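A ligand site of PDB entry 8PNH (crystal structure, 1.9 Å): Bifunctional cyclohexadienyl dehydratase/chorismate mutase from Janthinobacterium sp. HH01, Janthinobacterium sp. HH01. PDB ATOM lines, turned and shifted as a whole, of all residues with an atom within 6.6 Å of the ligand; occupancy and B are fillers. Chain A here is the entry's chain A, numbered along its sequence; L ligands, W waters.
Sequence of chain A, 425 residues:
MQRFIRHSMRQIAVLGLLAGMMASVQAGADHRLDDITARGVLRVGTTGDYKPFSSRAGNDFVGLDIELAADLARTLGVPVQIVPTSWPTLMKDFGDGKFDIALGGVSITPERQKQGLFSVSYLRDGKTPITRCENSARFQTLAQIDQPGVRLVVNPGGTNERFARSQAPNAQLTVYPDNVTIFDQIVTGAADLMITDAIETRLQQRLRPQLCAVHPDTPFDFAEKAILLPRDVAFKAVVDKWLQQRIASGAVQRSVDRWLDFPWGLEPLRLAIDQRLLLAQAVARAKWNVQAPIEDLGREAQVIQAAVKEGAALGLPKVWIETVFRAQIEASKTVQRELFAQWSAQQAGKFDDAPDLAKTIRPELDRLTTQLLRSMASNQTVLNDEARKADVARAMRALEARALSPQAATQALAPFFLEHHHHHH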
ATOM      1  N   ASP A  49     -30.973  -8.609  -2.969  1.00  0.00           N
ATOM      2  CA  ASP A  49     -32.231  -9.332  -2.907  1.00  0.00           C
ATOM      3  C   ASP A  49     -31.971 -10.834  -2.733  1.00  0.00           C
ATOM      4  O   ASP A  49     -32.671 -11.627  -3.344  1.00  0.00           O
ATOM      5  CB  ASP A  49     -33.068  -9.049  -4.151  1.00  0.00           C
ATOM      6  CG  ASP A  49     -32.654  -9.877  -5.367  1.00  0.00           C
ATOM      7  OD1 ASP A  49     -31.488  -9.717  -5.819  1.00  0.00           O
ATOM      8  OD2 ASP A  49     -33.486 -10.724  -5.814  1.00  0.00           O
ATOM      9  N   TYR A  50     -30.983 -11.216  -1.915  1.00  0.00           N
ATOM     10  CA  TYR A  50     -30.694 -12.626  -1.704  1.00  0.00           C
ATOM     11  C   TYR A  50     -30.252 -12.833  -0.261  1.00  0.00           C
ATOM     12  O   TYR A  50     -29.056 -12.939   0.022  1.00  0.00           O
ATOM     13  CB  TYR A  50     -29.666 -13.189  -2.694  1.00  0.00           C
ATOM     14  CG  TYR A  50     -29.410 -14.683  -2.603  1.00  0.00           C
ATOM     15  CD1 TYR A  50     -30.156 -15.496  -1.752  1.00  0.00           C
ATOM     16  CD2 TYR A  50     -28.388 -15.288  -3.329  1.00  0.00           C
ATOM     17  CE1 TYR A  50     -29.915 -16.863  -1.635  1.00  0.00           C
ATOM     18  CE2 TYR A  50     -28.143 -16.652  -3.236  1.00  0.00           C
ATOM     19  CZ  TYR A  50     -28.909 -17.441  -2.377  1.00  0.00           C
ATOM     20  OH  TYR A  50     -28.708 -18.788  -2.239  1.00  0.00           O
ATOM     21  N   GLY A 104     -22.887 -11.331  -3.081  1.00  0.00           N
ATOM     22  CA  GLY A 104     -24.323 -11.450  -2.876  1.00  0.00           C
ATOM     23  C   GLY A 104     -24.824 -12.839  -3.233  1.00  0.00           C
ATOM     24  O   GLY A 104     -25.791 -12.979  -3.989  1.00  0.00           O
ATOM     25  N   GLY A 105     -24.165 -13.880  -2.698  1.00  0.00           N
ATOM     26  CA  GLY A 105     -24.485 -15.256  -3.020  1.00  0.00           C
ATOM     27  C   GLY A 105     -24.160 -15.577  -4.483  1.00  0.00           C
ATOM     28  O   GLY A 105     -24.876 -16.345  -5.126  1.00  0.00           O
ATOM     29  N   VAL A 106     -23.037 -15.036  -4.985  1.00  0.00           N
ATOM     30  CA  VAL A 106     -22.668 -15.212  -6.385  1.00  0.00           C
ATOM     31  C   VAL A 106     -22.040 -16.604  -6.587  1.00  0.00           C
ATOM     32  O   VAL A 106     -20.971 -16.908  -6.059  1.00  0.00           O
ATOM     33  CB  VAL A 106     -21.722 -14.097  -6.886  1.00  0.00           C
ATOM     34  CG1 VAL A 106     -21.268 -14.367  -8.313  1.00  0.00           C
ATOM     35  CG2 VAL A 106     -22.315 -12.700  -6.774  1.00  0.00           C
ATOM     36  N   SER A 107     -22.658 -17.418  -7.441  1.00  0.00           N
ATOM     37  CA  SER A 107     -22.077 -18.697  -7.837  1.00  0.00           C
ATOM     38  C   SER A 107     -21.015 -18.510  -8.923  1.00  0.00           C
ATOM     39  O   SER A 107     -21.147 -17.659  -9.788  1.00  0.00           O
ATOM     40  CB  SER A 107     -23.125 -19.632  -8.347  1.00  0.00           C
ATOM     41  OG  SER A 107     -24.088 -19.887  -7.345  1.00  0.00           O
ATOM     42  N   ILE A 108     -19.990 -19.352  -8.878  1.00  0.00           N
ATOM     43  CA  ILE A 108     -19.001 -19.426  -9.956  1.00  0.00           C
ATOM     44  C   ILE A 108     -19.686 -20.074 -11.158  1.00  0.00           C
ATOM     45  O   ILE A 108     -20.174 -21.172 -11.014  1.00  0.00           O
ATOM     46  CB  ILE A 108     -17.761 -20.232  -9.517  1.00  0.00           C
ATOM     47  CG1 ILE A 108     -17.050 -19.546  -8.338  1.00  0.00           C
ATOM     48  CG2 ILE A 108     -16.813 -20.507 -10.688  1.00  0.00           C
ATOM     49  CD1 ILE A 108     -15.834 -20.270  -7.801  1.00  0.00           C
ATOM     50  N   THR A 109     -19.784 -19.338 -12.274  1.00  0.00           N
ATOM     51  CA  THR A 109     -20.285 -19.833 -13.552  1.00  0.00           C
ATOM     52  C   THR A 109     -19.223 -19.535 -14.616  1.00  0.00           C
ATOM     53  O   THR A 109     -18.381 -18.652 -14.421  1.00  0.00           O
ATOM     54  CB  THR A 109     -21.629 -19.199 -13.925  1.00  0.00           C
ATOM     55  OG1 THR A 109     -21.389 -17.822 -14.217  1.00  0.00           O
ATOM     56  CG2 THR A 109     -22.678 -19.285 -12.832  1.00  0.00           C
ATOM     57  N   ARG A 112     -19.326 -15.796 -15.967  1.00  0.00           N
ATOM     58  CA  ARG A 112     -18.730 -14.858 -15.022  1.00  0.00           C
ATOM     59  C   ARG A 112     -17.203 -15.001 -14.973  1.00  0.00           C
ATOM     60  O   ARG A 112     -16.507 -13.993 -14.790  1.00  0.00           O
ATOM     61  CB  ARG A 112     -19.388 -15.057 -13.654  1.00  0.00           C
ATOM     62  CG  ARG A 112     -20.861 -14.701 -13.662  1.00  0.00           C
ATOM     63  CD  ARG A 112     -21.466 -15.074 -12.337  1.00  0.00           C
ATOM     64  NE  ARG A 112     -22.908 -14.879 -12.319  1.00  0.00           N
ATOM     65  CZ  ARG A 112     -23.737 -15.506 -11.491  1.00  0.00           C
ATOM     66  NH1 ARG A 112     -23.263 -16.293 -10.550  1.00  0.00           N
ATOM     67  NH2 ARG A 112     -25.043 -15.338 -11.601  1.00  0.00           N
ATOM     68  N   LYS A 127     -27.610 -27.981  -4.502  1.00  0.00           N
ATOM     69  CA  LYS A 127     -28.814 -27.713  -5.273  1.00  0.00           C
ATOM     70  C   LYS A 127     -29.911 -28.705  -4.848  1.00  0.00           C
ATOM     71  O   LYS A 127     -29.753 -29.912  -5.037  1.00  0.00           O
ATOM     72  CB  LYS A 127     -28.549 -27.893  -6.770  1.00  0.00           C
ATOM     73  CG  LYS A 127     -27.548 -26.906  -7.374  1.00  0.00           C
ATOM     74  CD  LYS A 127     -28.107 -25.490  -7.312  1.00  0.00           C
ATOM     75  CE  LYS A 127     -27.102 -24.390  -7.542  1.00  0.00           C
ATOM     76  NZ  LYS A 127     -27.559 -23.104  -6.993  1.00  0.00           N
ATOM     77  N   VAL A 154     -37.540 -20.730 -11.207  1.00  0.00           N
ATOM     78  CA  VAL A 154     -36.151 -20.511 -10.906  1.00  0.00           C
ATOM     79  C   VAL A 154     -35.842 -19.031 -11.170  1.00  0.00           C
ATOM     80  O   VAL A 154     -36.591 -18.359 -11.870  1.00  0.00           O
ATOM     81  CB  VAL A 154     -35.317 -21.463 -11.782  1.00  0.00           C
ATOM     82  CG1 VAL A 154     -35.203 -20.951 -13.204  1.00  0.00           C
ATOM     83  CG2 VAL A 154     -33.964 -21.718 -11.197  1.00  0.00           C
ATOM     84  N   ASN A 155     -34.748 -18.535 -10.570  1.00  0.00           N
ATOM     85  CA  ASN A 155     -34.165 -17.241 -10.895  1.00  0.00           C
ATOM     86  C   ASN A 155     -33.252 -17.351 -12.122  1.00  0.00           C
ATOM     87  O   ASN A 155     -32.656 -18.398 -12.369  1.00  0.00           O
ATOM     88  CB  ASN A 155     -33.330 -16.718  -9.721  1.00  0.00           C
ATOM     89  CG  ASN A 155     -32.304 -17.749  -9.299  1.00  0.00           C
ATOM     90  OD1 ASN A 155     -32.644 -18.886  -9.010  1.00  0.00           O
ATOM     91  ND2 ASN A 155     -31.033 -17.355  -9.271  1.00  0.00           N
ATOM     92  N   PRO A 156     -33.021 -16.254 -12.888  1.00  0.00           N
ATOM     93  CA  PRO A 156     -32.304 -16.323 -14.172  1.00  0.00           C
ATOM     94  C   PRO A 156     -30.782 -16.192 -14.111  1.00  0.00           C
ATOM     95  O   PRO A 156     -30.259 -15.537 -13.205  1.00  0.00           O
ATOM     96  CB  PRO A 156     -32.859 -15.089 -14.899  1.00  0.00           C
ATOM     97  CG  PRO A 156     -33.022 -14.073 -13.789  1.00  0.00           C
ATOM     98  CD  PRO A 156     -33.490 -14.889 -12.597  1.00  0.00           C
ATOM     99  N   GLY A 157     -30.080 -16.868 -15.036  1.00  0.00           N
ATOM    100  CA  GLY A 157     -28.707 -16.539 -15.420  1.00  0.00           C
ATOM    101  C   GLY A 157     -27.620 -17.197 -14.558  1.00  0.00           C
ATOM    102  O   GLY A 157     -26.448 -16.866 -14.716  1.00  0.00           O
ATOM    103  N   GLY A 158     -27.991 -18.157 -13.689  1.00  0.00           N
ATOM    104  CA  GLY A 158     -27.071 -18.719 -12.717  1.00  0.00           C
ATOM    105  C   GLY A 158     -27.099 -20.242 -12.739  1.00  0.00           C
ATOM    106  O   GLY A 158     -27.624 -20.850 -13.664  1.00  0.00           O
ATOM    107  N   THR A 159     -26.528 -20.877 -11.725  1.00  0.00           N
ATOM    108  CA  THR A 159     -26.520 -22.328 -11.648  1.00  0.00           C
ATOM    109  C   THR A 159     -27.952 -22.908 -11.543  1.00  0.00           C
ATOM    110  O   THR A 159     -28.149 -24.056 -11.928  1.00  0.00           O
ATOM    111  CB  THR A 159     -25.552 -22.769 -10.545  1.00  0.00           C
ATOM    112  OG1 THR A 159     -26.092 -22.339  -9.295  1.00  0.00           O
ATOM    113  CG2 THR A 159     -24.174 -22.178 -10.732  1.00  0.00           C
ATOM    114  N   ASN A 160     -28.929 -22.187 -10.966  1.00  0.00           N
ATOM    115  CA  ASN A 160     -30.255 -22.799 -10.763  1.00  0.00           C
ATOM    116  C   ASN A 160     -30.877 -23.033 -12.141  1.00  0.00           C
ATOM    117  O   ASN A 160     -31.478 -24.088 -12.406  1.00  0.00           O
ATOM    118  CB  ASN A 160     -31.176 -21.980  -9.852  1.00  0.00           C
ATOM    119  CG  ASN A 160     -30.741 -21.957  -8.407  1.00  0.00           C
ATOM    120  OD1 ASN A 160     -30.045 -22.869  -7.958  1.00  0.00           O
ATOM    121  ND2 ASN A 160     -31.232 -20.979  -7.647  1.00  0.00           N
ATOM    122  N   GLU A 161     -30.825 -22.008 -12.992  1.00  0.00           N
ATOM    123  CA  GLU A 161     -31.409 -22.120 -14.314  1.00  0.00           C
ATOM    124  C   GLU A 161     -30.656 -23.159 -15.168  1.00  0.00           C
ATOM    125  O   GLU A 161     -31.277 -23.968 -15.860  1.00  0.00           O
ATOM    126  CB  GLU A 161     -31.512 -20.722 -14.943  1.00  0.00           C
ATOM    127  CG  GLU A 161     -31.923 -20.763 -16.403  1.00  0.00           C
ATOM    128  CD  GLU A 161     -32.290 -19.432 -17.063  1.00  0.00           C
ATOM    129  OE1 GLU A 161     -31.697 -18.394 -16.731  1.00  0.00           O
ATOM    130  OE2 GLU A 161     -33.156 -19.464 -17.925  1.00  0.00           O
ATOM    131  N   ASN A 179     -36.908 -12.434  -6.094  1.00  0.00           N
ATOM    132  CA  ASN A 179     -36.961 -13.465  -5.061  1.00  0.00           C
ATOM    133  C   ASN A 179     -38.408 -13.612  -4.553  1.00  0.00           C
ATOM    134  O   ASN A 179     -39.056 -14.650  -4.732  1.00  0.00           O
ATOM    135  CB  ASN A 179     -35.957 -13.082  -3.960  1.00  0.00           C
ATOM    136  CG  ASN A 179     -35.361 -14.250  -3.210  1.00  0.00           C
ATOM    137  OD1 ASN A 179     -34.346 -14.810  -3.627  1.00  0.00           O
ATOM    138  ND2 ASN A 179     -35.961 -14.575  -2.073  1.00  0.00           N
ATOM    139  N   PHE A 183     -41.061 -17.314  -4.212  1.00  0.00           N
ATOM    140  CA  PHE A 183     -41.539 -17.986  -3.020  1.00  0.00           C
ATOM    141  C   PHE A 183     -43.040 -17.754  -2.832  1.00  0.00           C
ATOM    142  O   PHE A 183     -43.717 -18.674  -2.392  1.00  0.00           O
ATOM    143  CB  PHE A 183     -40.689 -17.610  -1.816  1.00  0.00           C
ATOM    144  CG  PHE A 183     -39.302 -18.117  -2.003  1.00  0.00           C
ATOM    145  CD1 PHE A 183     -39.079 -19.474  -2.092  1.00  0.00           C
ATOM    146  CD2 PHE A 183     -38.248 -17.239  -2.262  1.00  0.00           C
ATOM    147  CE1 PHE A 183     -37.807 -19.965  -2.379  1.00  0.00           C
ATOM    148  CE2 PHE A 183     -36.984 -17.738  -2.519  1.00  0.00           C
ATOM    149  CZ  PHE A 183     -36.765 -19.088  -2.603  1.00  0.00           C
ATOM    150  N   MET A 194     -39.105 -24.902  -6.382  1.00  0.00           N
ATOM    151  CA  MET A 194     -37.887 -24.318  -6.906  1.00  0.00           C
ATOM    152  C   MET A 194     -36.743 -25.260  -6.524  1.00  0.00           C
ATOM    153  O   MET A 194     -36.804 -25.871  -5.474  1.00  0.00           O
ATOM    154  CB  MET A 194     -37.722 -22.926  -6.303  1.00  0.00           C
ATOM    155  CG  MET A 194     -36.516 -22.148  -6.829  1.00  0.00           C
ATOM    156  SD  MET A 194     -36.037 -20.795  -5.792  1.00  0.00           S
ATOM    157  CE  MET A 194     -34.833 -20.000  -6.854  1.00  0.00           C
ATOM    158  N   THR A 196     -32.881 -24.765  -5.688  1.00  0.00           N
ATOM    159  CA  THR A 196     -32.027 -23.619  -5.379  1.00  0.00           C
ATOM    160  C   THR A 196     -30.900 -24.041  -4.423  1.00  0.00           C
ATOM    161  O   THR A 196     -30.800 -25.212  -4.066  1.00  0.00           O
ATOM    162  CB  THR A 196     -32.876 -22.435  -4.881  1.00  0.00           C
ATOM    163  OG1 THR A 196     -32.004 -21.311  -4.739  1.00  0.00           O
ATOM    164  CG2 THR A 196     -33.610 -22.670  -3.576  1.00  0.00           C
ATOM    165  N   ASP A 197     -30.060 -23.077  -4.001  1.00  0.00           N
ATOM    166  CA  ASP A 197     -29.070 -23.347  -2.985  1.00  0.00           C
ATOM    167  C   ASP A 197     -29.713 -23.867  -1.693  1.00  0.00           C
ATOM    168  O   ASP A 197     -30.630 -23.244  -1.176  1.00  0.00           O
ATOM    169  CB  ASP A 197     -28.233 -22.128  -2.623  1.00  0.00           C
ATOM    170  CG  ASP A 197     -27.526 -21.577  -3.852  1.00  0.00           C
ATOM    171  OD1 ASP A 197     -26.962 -22.383  -4.595  1.00  0.00           O
ATOM    172  OD2 ASP A 197     -27.607 -20.357  -4.082  1.00  0.00           O
ATOM    173  N   GLU A 200     -30.630 -21.293   0.929  1.00  0.00           N
ATOM    174  CA  GLU A 200     -31.867 -20.587   0.711  1.00  0.00           C
ATOM    175  C   GLU A 200     -33.056 -21.438   1.185  1.00  0.00           C
ATOM    176  O   GLU A 200     -33.987 -20.883   1.765  1.00  0.00           O
ATOM    177  CB  GLU A 200     -31.990 -20.168  -0.761  1.00  0.00           C
ATOM    178  CG  GLU A 200     -33.208 -19.290  -1.025  1.00  0.00           C
ATOM    179  CD  GLU A 200     -33.136 -18.536  -2.340  1.00  0.00           C
ATOM    180  OE1 GLU A 200     -32.885 -19.199  -3.370  1.00  0.00           O
ATOM    181  OE2 GLU A 200     -33.299 -17.308  -2.324  1.00  0.00           O
ATOM    182  N   ALA A 223     -22.857 -26.062  -5.762  1.00  0.00           N
ATOM    183  CA  ALA A 223     -22.333 -24.829  -6.334  1.00  0.00           C
ATOM    184  C   ALA A 223     -21.375 -24.161  -5.338  1.00  0.00           C
ATOM    185  O   ALA A 223     -21.478 -24.336  -4.131  1.00  0.00           O
ATOM    186  CB  ALA A 223     -23.473 -23.907  -6.700  1.00  0.00           C
ATOM    187  N   LYS A 225     -19.943 -20.563  -3.867  1.00  0.00           N
ATOM    188  CA  LYS A 225     -20.109 -19.120  -3.729  1.00  0.00           C
ATOM    189  C   LYS A 225     -18.730 -18.498  -3.600  1.00  0.00           C
ATOM    190  O   LYS A 225     -17.885 -19.044  -2.892  1.00  0.00           O
ATOM    191  CB  LYS A 225     -21.001 -18.794  -2.537  1.00  0.00           C
ATOM    192  CG  LYS A 225     -22.373 -19.471  -2.563  1.00  0.00           C
ATOM    193  CD  LYS A 225     -23.193 -19.092  -3.788  1.00  0.00           C
ATOM    194  CE  LYS A 225     -24.643 -19.526  -3.672  1.00  0.00           C
ATOM    195  NZ  LYS A 225     -25.466 -19.116  -4.843  1.00  0.00           N
HETATM  196  C1  LIG L   1     -26.868 -18.602  -9.047  1.00  0.00           C
HETATM  197  O1  LIG L   1     -26.417 -19.507  -9.683  1.00  0.00           O
HETATM  198  O2  LIG L   1     -26.192 -17.648  -8.720  1.00  0.00           O
HETATM  199  C2  LIG L   1     -28.029 -18.787  -8.526  1.00  0.00           C
HETATM  200  O3  LIG L   1     -28.884 -19.304  -9.244  1.00  0.00           O
HETATM  201  C3  LIG L   1     -28.251 -18.653  -6.999  1.00  0.00           C
HETATM  202  C4  LIG L   1     -29.383 -17.784  -6.479  1.00  0.00           C
HETATM  203  C5  LIG L   1     -30.347 -18.318  -5.641  1.00  0.00           C
HETATM  204  C6  LIG L   1     -31.384 -17.531  -5.161  1.00  0.00           C
HETATM  205  C7  LIG L   1     -31.453 -16.197  -5.475  1.00  0.00           C
HETATM  206  C8  LIG L   1     -30.501 -15.652  -6.297  1.00  0.00           C
HETATM  207  C9  LIG L   1     -29.464 -16.439  -6.777  1.00  0.00           C
HETATM  208  O   HOH W   1     -30.147 -19.214 -12.087  1.00  0.00           O
HETATM  209  O   HOH W   2     -30.838 -12.442  -7.298  1.00  0.00           O
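Tyr 50 touches the ligand.
Arg 112 touches the ligand (NH1 to O2, 3.7 Å).
CA of Gly 158 touches O1 of the ligand, at 3.2 Å.
OD1 of Asn 179 touches C7 of the ligand, at 3.7 Å.
OG1 of Thr 196 touches C5 of the ligand (3.5 Å).
OD2 of Asp 197 touches C3 of the ligand, at 3.4 Å.
Glu 200 touches the ligand.
NZ of Lys 225 touches C3 of the ligand, at 3.6 Å.
Hydrophobic or aromatic side chains within 4 Å of the ligand: Tyr 50.
Of the 26 residues printed, 12 come within 4 Å of the ligand.
The nearest printed residue that does not touch the ligand is Gly 105 (4.04 Å).
An oxygen (O1) of the ligand lies within hydrogen-bond range of the backbone NH (N) of Thr 159, 2.5 Å away.
The side-chain hydroxyl of Thr 159 lies within hydrogen-bond range of an oxygen (O1) of the ligand (2.9 Å).
The side-chain amide nitrogen of Asn 155 is in hydrogen-bond range of an oxygen (O3) of the ligand, at 2.9 Å.
N of Asn 160 sits close to O3 of the ligand (3.4 Å).
An oxygen (O3) of the ligand lies within hydrogen-bond range of the side-chain amide nitrogen (ND2) of Asn 160, 3.3 Å away.
The side-chain hydroxyl (OG) of Ser 107 sits at hydrogen-bond distance from an oxygen (O1) of the ligand (3.3 Å).
OG1 of Thr 196 lies within hydrogen-bond range of OE1 of Glu 200 (2.7 Å).
OD1 of Asn 155 is in hydrogen-bond range of ND2 of Asn 160, at 2.9 Å.
The side-chain amino group (NZ) of Lys 225 sits at hydrogen-bond distance from the side-chain hydroxyl (OG) of Ser 107.
The backbone carbonyl oxygen (O) of Ser 107 sits at hydrogen-bond distance from the guanidinium group (NH1) of Arg 112, at 2.6 Å.
OD2 of Asp 197 sits at hydrogen-bond distance from OH of Tyr 50 (2.7 Å).
The side-chain carboxylate of Asp 197 is in salt-bridge range of the side-chain amino group of Lys 127 (2.6 Å).
The side-chain amino group (NZ) of Lys 225 sits at hydrogen-bond distance from the backbone carbonyl oxygen (O) of Gly 105 (2.8 Å).
The side-chain hydroxyl (OG1) of Thr 109 lies close to the backbone NH (N) of Arg 112.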
